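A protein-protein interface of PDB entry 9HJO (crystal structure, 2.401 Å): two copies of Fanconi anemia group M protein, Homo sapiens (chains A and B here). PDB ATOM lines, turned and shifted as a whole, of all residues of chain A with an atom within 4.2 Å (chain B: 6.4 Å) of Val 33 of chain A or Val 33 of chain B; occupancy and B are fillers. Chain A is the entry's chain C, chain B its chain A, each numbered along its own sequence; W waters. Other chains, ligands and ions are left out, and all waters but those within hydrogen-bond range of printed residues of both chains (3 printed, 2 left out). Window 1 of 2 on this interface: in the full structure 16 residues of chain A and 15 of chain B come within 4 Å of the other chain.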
ATOM      1  N   VAL A   8     -22.041  -9.797  23.870  1.00  0.00           N
ATOM      2  CA  VAL A   8     -22.793 -10.711  23.041  1.00  0.00           C
ATOM      3  C   VAL A   8     -22.660 -12.116  23.608  1.00  0.00           C
ATOM      4  O   VAL A   8     -21.537 -12.565  23.888  1.00  0.00           O
ATOM      5  CB  VAL A   8     -22.181 -10.639  21.634  1.00  0.00           C
ATOM      6  CG1 VAL A   8     -22.878 -11.586  20.658  1.00  0.00           C
ATOM      7  CG2 VAL A   8     -22.176  -9.194  21.131  1.00  0.00           C
ATOM      8  N   GLY A  10     -22.224 -16.015  23.462  1.00  0.00           N
ATOM      9  CA  GLY A  10     -21.479 -16.860  22.544  1.00  0.00           C
ATOM     10  C   GLY A  10     -22.374 -17.598  21.543  1.00  0.00           C
ATOM     11  O   GLY A  10     -21.959 -17.838  20.415  1.00  0.00           O
ATOM     12  N   ILE A  13     -23.054 -16.701  17.703  1.00  0.00           N
ATOM     13  CA  ILE A  13     -22.219 -17.028  16.549  1.00  0.00           C
ATOM     14  C   ILE A  13     -22.866 -18.117  15.694  1.00  0.00           C
ATOM     15  O   ILE A  13     -22.451 -18.289  14.560  1.00  0.00           O
ATOM     16  CB  ILE A  13     -20.767 -17.380  16.955  1.00  0.00           C
ATOM     17  CG1 ILE A  13     -20.653 -18.727  17.650  1.00  0.00           C
ATOM     18  CG2 ILE A  13     -20.173 -16.261  17.813  1.00  0.00           C
ATOM     19  CD1 ILE A  13     -19.237 -19.130  17.985  1.00  0.00           C
ATOM     20  N   LEU A  17     -23.729 -13.858  13.080  1.00  0.00           N
ATOM     21  CA  LEU A  17     -22.377 -13.453  12.685  1.00  0.00           C
ATOM     22  C   LEU A  17     -22.343 -12.071  12.041  1.00  0.00           C
ATOM     23  O   LEU A  17     -21.370 -11.360  12.248  1.00  0.00           O
ATOM     24  CB  LEU A  17     -21.672 -14.449  11.773  1.00  0.00           C
ATOM     25  CG  LEU A  17     -21.504 -15.848  12.357  1.00  0.00           C
ATOM     26  CD1 LEU A  17     -21.131 -16.774  11.249  1.00  0.00           C
ATOM     27  CD2 LEU A  17     -20.494 -15.870  13.478  1.00  0.00           C
ATOM     28  N   ARG A  24     -18.912  -4.323  15.366  1.00  0.00           N
ATOM     29  CA  ARG A  24     -17.498  -3.964  15.373  1.00  0.00           C
ATOM     30  C   ARG A  24     -17.228  -2.931  14.286  1.00  0.00           C
ATOM     31  O   ARG A  24     -16.754  -1.842  14.576  1.00  0.00           O
ATOM     32  CB  ARG A  24     -16.499  -5.085  15.063  1.00  0.00           C
ATOM     33  CG  ARG A  24     -16.514  -6.256  16.023  1.00  0.00           C
ATOM     34  CD  ARG A  24     -15.503  -7.325  15.618  1.00  0.00           C
ATOM     35  NE  ARG A  24     -15.855  -8.594  16.268  1.00  0.00           N
ATOM     36  CZ  ARG A  24     -15.835  -8.792  17.589  1.00  0.00           C
ATOM     37  NH1 ARG A  24     -16.221  -9.949  18.109  1.00  0.00           N
ATOM     38  NH2 ARG A  24     -15.365  -7.851  18.396  1.00  0.00           N
ATOM     39  N   GLU A  32     -17.529  -7.684  22.575  1.00  0.00           N
ATOM     40  CA  GLU A  32     -16.912  -8.889  23.072  1.00  0.00           C
ATOM     41  C   GLU A  32     -17.960 -10.007  23.140  1.00  0.00           C
ATOM     42  O   GLU A  32     -19.076  -9.818  23.620  1.00  0.00           O
ATOM     43  CB  GLU A  32     -16.138  -8.531  24.338  1.00  0.00           C
ATOM     44  CG  GLU A  32     -15.178  -9.650  24.744  1.00  0.00           C
ATOM     45  CD  GLU A  32     -13.915  -9.253  25.484  1.00  0.00           C
ATOM     46  OE1 GLU A  32     -13.212  -8.379  24.958  1.00  0.00           O
ATOM     47  OE2 GLU A  32     -13.595  -9.860  26.525  1.00  0.00           O
ATOM     48  N   VAL A  33     -17.563 -11.177  22.630  1.00  0.00           N
ATOM     49  CA  VAL A  33     -18.368 -12.384  22.618  1.00  0.00           C
ATOM     50  C   VAL A  33     -18.046 -13.123  23.914  1.00  0.00           C
ATOM     51  O   VAL A  33     -16.900 -13.482  24.136  1.00  0.00           O
ATOM     52  CB  VAL A  33     -17.996 -13.205  21.360  1.00  0.00           C
ATOM     53  CG1 VAL A  33     -18.660 -14.568  21.329  1.00  0.00           C
ATOM     54  CG2 VAL A  33     -18.280 -12.424  20.084  1.00  0.00           C
ATOM     55  N   CME A  34     -19.068 -13.370  24.731  1.00  0.00           N
ATOM     56  CA  CME A  34     -18.917 -13.729  26.133  1.00  0.00           C
ATOM     57  CB  CME A  34     -19.327 -12.591  27.050  1.00  0.00           C
ATOM     58  SG  CME A  34     -18.368 -11.074  26.800  1.00  0.00           S
ATOM     59  SD  CME A  34     -16.557 -11.535  27.552  1.00  0.00           S
ATOM     60  CE  CME A  34     -16.446 -10.570  29.087  1.00  0.00           C
ATOM     61  CZ  CME A  34     -15.606  -9.332  28.918  1.00  0.00           C
ATOM     62  OH  CME A  34     -14.264  -9.535  29.384  1.00  0.00           O
ATOM     63  C   CME A  34     -19.735 -14.978  26.426  1.00  0.00           C
ATOM     64  O   CME A  34     -20.831 -15.128  25.881  1.00  0.00           O
ATOM     65  N   ILE B   6      -8.040 -14.364  11.251  1.00  0.00           N
ATOM     66  CA  ILE B   6      -7.910 -15.583  12.025  1.00  0.00           C
ATOM     67  C   ILE B   6      -9.276 -15.941  12.576  1.00  0.00           C
ATOM     68  O   ILE B   6     -10.014 -15.067  13.036  1.00  0.00           O
ATOM     69  CB  ILE B   6      -6.839 -15.466  13.123  1.00  0.00           C
ATOM     70  CG1 ILE B   6      -6.746 -16.714  13.953  1.00  0.00           C
ATOM     71  CG2 ILE B   6      -7.069 -14.250  14.009  1.00  0.00           C
ATOM     72  CD1 ILE B   6      -5.421 -16.831  14.656  1.00  0.00           C
ATOM     73  N   LEU B   7      -9.580 -17.240  12.512  1.00  0.00           N
ATOM     74  CA  LEU B   7     -10.825 -17.759  13.028  1.00  0.00           C
ATOM     75  C   LEU B   7     -10.520 -18.460  14.344  1.00  0.00           C
ATOM     76  O   LEU B   7      -9.575 -19.245  14.426  1.00  0.00           O
ATOM     77  CB  LEU B   7     -11.462 -18.692  12.003  1.00  0.00           C
ATOM     78  CG  LEU B   7     -11.546 -18.142  10.574  1.00  0.00           C
ATOM     79  CD1 LEU B   7     -12.251 -19.169   9.731  1.00  0.00           C
ATOM     80  CD2 LEU B   7     -12.262 -16.806  10.538  1.00  0.00           C
ATOM     81  N   VAL B   8     -11.381 -18.177  15.327  1.00  0.00           N
ATOM     82  CA  VAL B   8     -11.328 -18.704  16.672  1.00  0.00           C
ATOM     83  C   VAL B   8     -12.573 -19.542  16.932  1.00  0.00           C
ATOM     84  O   VAL B   8     -13.686 -19.080  16.668  1.00  0.00           O
ATOM     85  CB  VAL B   8     -11.303 -17.477  17.603  1.00  0.00           C
ATOM     86  CG1 VAL B   8     -11.280 -17.874  19.076  1.00  0.00           C
ATOM     87  CG2 VAL B   8     -10.164 -16.535  17.231  1.00  0.00           C
ATOM     88  N   GLY B   9     -12.391 -20.740  17.487  1.00  0.00           N
ATOM     89  CA  GLY B   9     -13.524 -21.527  17.945  1.00  0.00           C
ATOM     90  C   GLY B   9     -14.282 -20.835  19.089  1.00  0.00           C
ATOM     91  O   GLY B   9     -13.699 -20.228  19.995  1.00  0.00           O
ATOM     92  N   GLY B  10     -15.604 -20.898  19.035  1.00  0.00           N
ATOM     93  CA  GLY B  10     -16.446 -20.260  20.033  1.00  0.00           C
ATOM     94  C   GLY B  10     -16.151 -20.713  21.464  1.00  0.00           C
ATOM     95  O   GLY B  10     -16.306 -19.931  22.383  1.00  0.00           O
ATOM     96  N   HIS B  11     -15.756 -21.977  21.646  1.00  0.00           N
ATOM     97  CA  HIS B  11     -15.409 -22.539  22.946  1.00  0.00           C
ATOM     98  C   HIS B  11     -14.280 -21.765  23.630  1.00  0.00           C
ATOM     99  O   HIS B  11     -14.225 -21.769  24.838  1.00  0.00           O
ATOM    100  CB  HIS B  11     -15.044 -24.024  22.832  1.00  0.00           C
ATOM    101  CG  HIS B  11     -13.901 -24.322  21.909  1.00  0.00           C
ATOM    102  ND1 HIS B  11     -14.132 -24.444  20.565  1.00  0.00           N
ATOM    103  CD2 HIS B  11     -12.562 -24.502  22.064  1.00  0.00           C
ATOM    104  CE1 HIS B  11     -12.996 -24.714  19.951  1.00  0.00           C
ATOM    105  NE2 HIS B  11     -12.023 -24.732  20.816  1.00  0.00           N
ATOM    106  N   ILE B  13     -14.059 -18.712  24.200  1.00  0.00           N
ATOM    107  CA  ILE B  13     -14.531 -17.648  25.086  1.00  0.00           C
ATOM    108  C   ILE B  13     -14.653 -18.129  26.537  1.00  0.00           C
ATOM    109  O   ILE B  13     -14.732 -17.293  27.423  1.00  0.00           O
ATOM    110  CB  ILE B  13     -15.838 -16.993  24.576  1.00  0.00           C
ATOM    111  CG1 ILE B  13     -17.057 -17.894  24.749  1.00  0.00           C
ATOM    112  CG2 ILE B  13     -15.650 -16.536  23.124  1.00  0.00           C
ATOM    113  CD1 ILE B  13     -18.344 -17.272  24.261  1.00  0.00           C
ATOM    114  N   LEU B  17     -10.355 -15.439  26.563  1.00  0.00           N
ATOM    115  CA  LEU B  17     -10.835 -14.083  26.299  1.00  0.00           C
ATOM    116  C   LEU B  17      -9.695 -13.104  26.060  1.00  0.00           C
ATOM    117  O   LEU B  17      -9.883 -12.195  25.270  1.00  0.00           O
ATOM    118  CB  LEU B  17     -11.758 -13.522  27.369  1.00  0.00           C
ATOM    119  CG  LEU B  17     -13.021 -14.332  27.615  1.00  0.00           C
ATOM    120  CD1 LEU B  17     -13.647 -13.839  28.877  1.00  0.00           C
ATOM    121  CD2 LEU B  17     -13.997 -14.244  26.452  1.00  0.00           C
ATOM    122  N   ILE B  20      -8.186 -13.699  22.510  1.00  0.00           N
ATOM    123  CA  ILE B  20      -9.058 -13.159  21.480  1.00  0.00           C
ATOM    124  C   ILE B  20      -8.887 -11.651  21.401  1.00  0.00           C
ATOM    125  O   ILE B  20      -8.650 -11.144  20.309  1.00  0.00           O
ATOM    126  CB  ILE B  20     -10.516 -13.576  21.732  1.00  0.00           C
ATOM    127  CG1 ILE B  20     -10.673 -15.070  21.504  1.00  0.00           C
ATOM    128  CG2 ILE B  20     -11.513 -12.779  20.883  1.00  0.00           C
ATOM    129  CD1 ILE B  20     -11.786 -15.678  22.325  1.00  0.00           C
ATOM    130  N   ARG B  24      -7.269  -8.906  18.376  1.00  0.00           N
ATOM    131  CA  ARG B  24      -7.931  -7.739  17.799  1.00  0.00           C
ATOM    132  C   ARG B  24      -7.078  -6.500  18.045  1.00  0.00           C
ATOM    133  O   ARG B  24      -6.689  -5.825  17.106  1.00  0.00           O
ATOM    134  CB  ARG B  24      -9.300  -7.356  18.373  1.00  0.00           C
ATOM    135  CG  ARG B  24     -10.358  -8.439  18.278  1.00  0.00           C
ATOM    136  CD  ARG B  24     -11.688  -7.989  18.863  1.00  0.00           C
ATOM    137  NE  ARG B  24     -12.508  -9.176  19.118  1.00  0.00           N
ATOM    138  CZ  ARG B  24     -13.007  -9.967  18.163  1.00  0.00           C
ATOM    139  NH1 ARG B  24     -13.698 -11.075  18.451  1.00  0.00           N
ATOM    140  NH2 ARG B  24     -12.860  -9.619  16.895  1.00  0.00           N
ATOM    141  N   VAL B  31     -10.418 -10.683  13.696  1.00  0.00           N
ATOM    142  CA  VAL B  31     -10.590 -11.877  14.493  1.00  0.00           C
ATOM    143  C   VAL B  31     -12.076 -12.167  14.509  1.00  0.00           C
ATOM    144  O   VAL B  31     -12.858 -11.325  14.948  1.00  0.00           O
ATOM    145  CB  VAL B  31     -10.029 -11.735  15.917  1.00  0.00           C
ATOM    146  CG1 VAL B  31     -10.284 -12.992  16.746  1.00  0.00           C
ATOM    147  CG2 VAL B  31      -8.548 -11.348  15.930  1.00  0.00           C
ATOM    148  N   GLU B  32     -12.458 -13.349  14.047  1.00  0.00           N
ATOM    149  CA  GLU B  32     -13.853 -13.716  14.130  1.00  0.00           C
ATOM    150  C   GLU B  32     -13.966 -15.003  14.947  1.00  0.00           C
ATOM    151  O   GLU B  32     -13.250 -15.982  14.705  1.00  0.00           O
ATOM    152  CB  GLU B  32     -14.523 -13.650  12.755  1.00  0.00           C
ATOM    153  CG  GLU B  32     -16.042 -13.729  12.849  1.00  0.00           C
ATOM    154  CD  GLU B  32     -16.883 -13.060  11.787  1.00  0.00           C
ATOM    155  OE1 GLU B  32     -16.598 -13.387  10.636  1.00  0.00           O
ATOM    156  OE2 GLU B  32     -17.826 -12.278  12.121  1.00  0.00           O
ATOM    157  N   VAL B  33     -14.883 -14.961  15.926  1.00  0.00           N
ATOM    158  CA  VAL B  33     -15.239 -16.087  16.765  1.00  0.00           C
ATOM    159  C   VAL B  33     -16.343 -16.850  16.029  1.00  0.00           C
ATOM    160  O   VAL B  33     -17.378 -16.269  15.719  1.00  0.00           O
ATOM    161  CB  VAL B  33     -15.689 -15.535  18.136  1.00  0.00           C
ATOM    162  CG1 VAL B  33     -16.328 -16.588  19.026  1.00  0.00           C
ATOM    163  CG2 VAL B  33     -14.546 -14.827  18.834  1.00  0.00           C
ATOM    164  N   CME B  34     -16.109 -18.146  15.802  1.00  0.00           N
ATOM    165  CA  CME B  34     -16.821 -18.941  14.821  1.00  0.00           C
ATOM    166  CB  CME B  34     -15.962 -19.229  13.586  1.00  0.00           C
ATOM    167  SG  CME B  34     -15.429 -17.735  12.719  1.00  0.00           S
ATOM    168  SD  CME B  34     -17.131 -17.116  11.831  1.00  0.00           S
ATOM    169  CE  CME B  34     -16.637 -17.170  10.076  1.00  0.00           C
ATOM    170  CZ  CME B  34     -17.730 -16.805   9.111  1.00  0.00           C
ATOM    171  OH  CME B  34     -17.728 -15.431   8.743  1.00  0.00           O
ATOM    172  C   CME B  34     -17.277 -20.242  15.453  1.00  0.00           C
ATOM    173  O   CME B  34     -16.537 -20.801  16.263  1.00  0.00           O
ATOM    174  N   PRO B  35     -18.389 -20.844  14.968  1.00  0.00           N
ATOM    175  CA  PRO B  35     -18.779 -22.185  15.370  1.00  0.00           C
ATOM    176  C   PRO B  35     -17.944 -23.296  14.737  1.00  0.00           C
ATOM    177  O   PRO B  35     -18.445 -24.153  14.029  1.00  0.00           O
ATOM    178  CB  PRO B  35     -20.240 -22.191  14.958  1.00  0.00           C
ATOM    179  CG  PRO B  35     -20.146 -21.443  13.634  1.00  0.00           C
ATOM    180  CD  PRO B  35     -19.322 -20.266  13.984  1.00  0.00           C
HETATM  181  O   HOH W   1     -12.811  -9.376  22.476  1.00  0.00           O
HETATM  182  O   HOH W   2     -12.444 -11.496  24.162  1.00  0.00           O
HETATM  183  O   HOH W   3     -16.982 -10.681  14.101  1.00  0.00           O
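The guanidinium group of Arg 24 of chain A sits close to the guanidinium group of Arg 24 of chain B, at 2.8 Å.
The guanidinium group (NH2) of Arg 24 of chain B lies within hydrogen-bond range of the backbone carbonyl oxygen (O) of Val 31 of chain B.
The backbone carbonyl oxygen (O) of Glu 32 of chain B is in hydrogen-bond range of the backbone NH (N) of Val 8 of chain B, at 2.9 Å.
The backbone NH (N) of Gly 10 of chain B is in hydrogen-bond range of O of CME 34 of chain B, at 2.9 Å.
O of Val 8 of chain B is in hydrogen-bond range of N of CME 34 of chain B (2.7 Å).
The backbone carbonyl oxygen (O) of Ile 6 of chain B is in hydrogen-bond range of the backbone NH (N) of Glu 32 of chain B (3.2 Å).
OH of CME 34 of chain B sits at hydrogen-bond distance from the side-chain carboxylate (OE1) of Glu 32 of chain B (3.0 Å).
CA of Gly 10 of chain A touches CD1 of Ile 13 of chain B, 3.6 Å away.
Ile 13 of chain A touches Gly 10 of chain B.
Ile 13 of chain A touches Val 33 of chain B.
Leu 17 of chain A touches Glu 32 of chain B (O to OE2, 3.7 Å).
Val 33 of chain B touches Leu 17 of chain A (O to CD2, 3.9 Å).
CD2 of Leu 17 of chain A touches SD of CME 34 of chain B, at 3.9 Å.
Val 33 of chain A touches Ile 13 of chain B (O to CG2, 3.5 Å).
Val 33 of chain A touches Leu 17 of chain B (O to CD2, 3.8 Å).
Ile 13 of chain B touches CME 34 of chain A (CD1 to C, 3.4 Å).
CME 34 of chain A touches Leu 17 of chain B.
Printed residues of chain B within 4 Å of Arg 24 of chain A: Arg 24 (2.8 Å).
Val 33 of chain A touches just these residues of chain B: Ile 13, Leu 17 and Val 33.
Of the printed residues of chain B, CME 34 of chain A touches Ile 13 (3.4 Å) and Leu 17 (3.9 Å).
Of the printed residues of chain A, Leu 17 of chain B touches Val 33 and CME 34.
Val 31 of chain B touches none of the printed residues of chain A.
Of the printed residues of chain A, Glu 32 of chain B touches Leu 17.
Val 33 of chain B touches three residues of chain A.
Of the printed residues of chain A, Pro 35 of chain B touches Ile 13 (3.6 Å).
The nearest printed residue of chain A that does not touch Val 33 of chain B is Arg 24 of chain A (5.2 Å).
The nearest printed residue of chain B that does not touch Gly 10 of chain A is Val 33 of chain B (5.9 Å).
Hydrophobic or aromatic side chains of chain A within 4 Å of the printed part of chain B: Ile 13, Leu 17 and Val 33.
Gly 10 of chain A touches Ile 13 of chain B, and with the chains exchanged Ile 13 of chain A touches Gly 10 of chain B.
Ile 13 of chain A touches Val 33 of chain B, and with the chains exchanged Val 33 of chain A touches Ile 13 of chain B.
Ile 13 of chain A touches CME 34 of chain B, and with the chains exchanged CME 34 of chain A touches Ile 13 of chain B.
Leu 17 of chain A touches Glu 32 of chain B, but with the chains exchanged Glu 32 of chain A does not touch Leu 17 of chain B (4.2 Å).
Positions printed for both chains: 8, 10, 13, 17, 24, 32, 33 and 34.
Water W3 bridges the side-chain carboxylate of Glu 32 of chain B (2.7 Å) and the guanidinium group of Arg 24 of chain A (3.2 Å).
Water W1 bridges the side-chain carboxylate of Glu 32 of chain A (2.7 Å) and the guanidinium group of Arg 24 of chain B (3.4 Å).
Water W2 bridges O of Leu 17 of chain B (2.9 Å) and OE2 of Glu 32 of chain A (3.1 Å).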
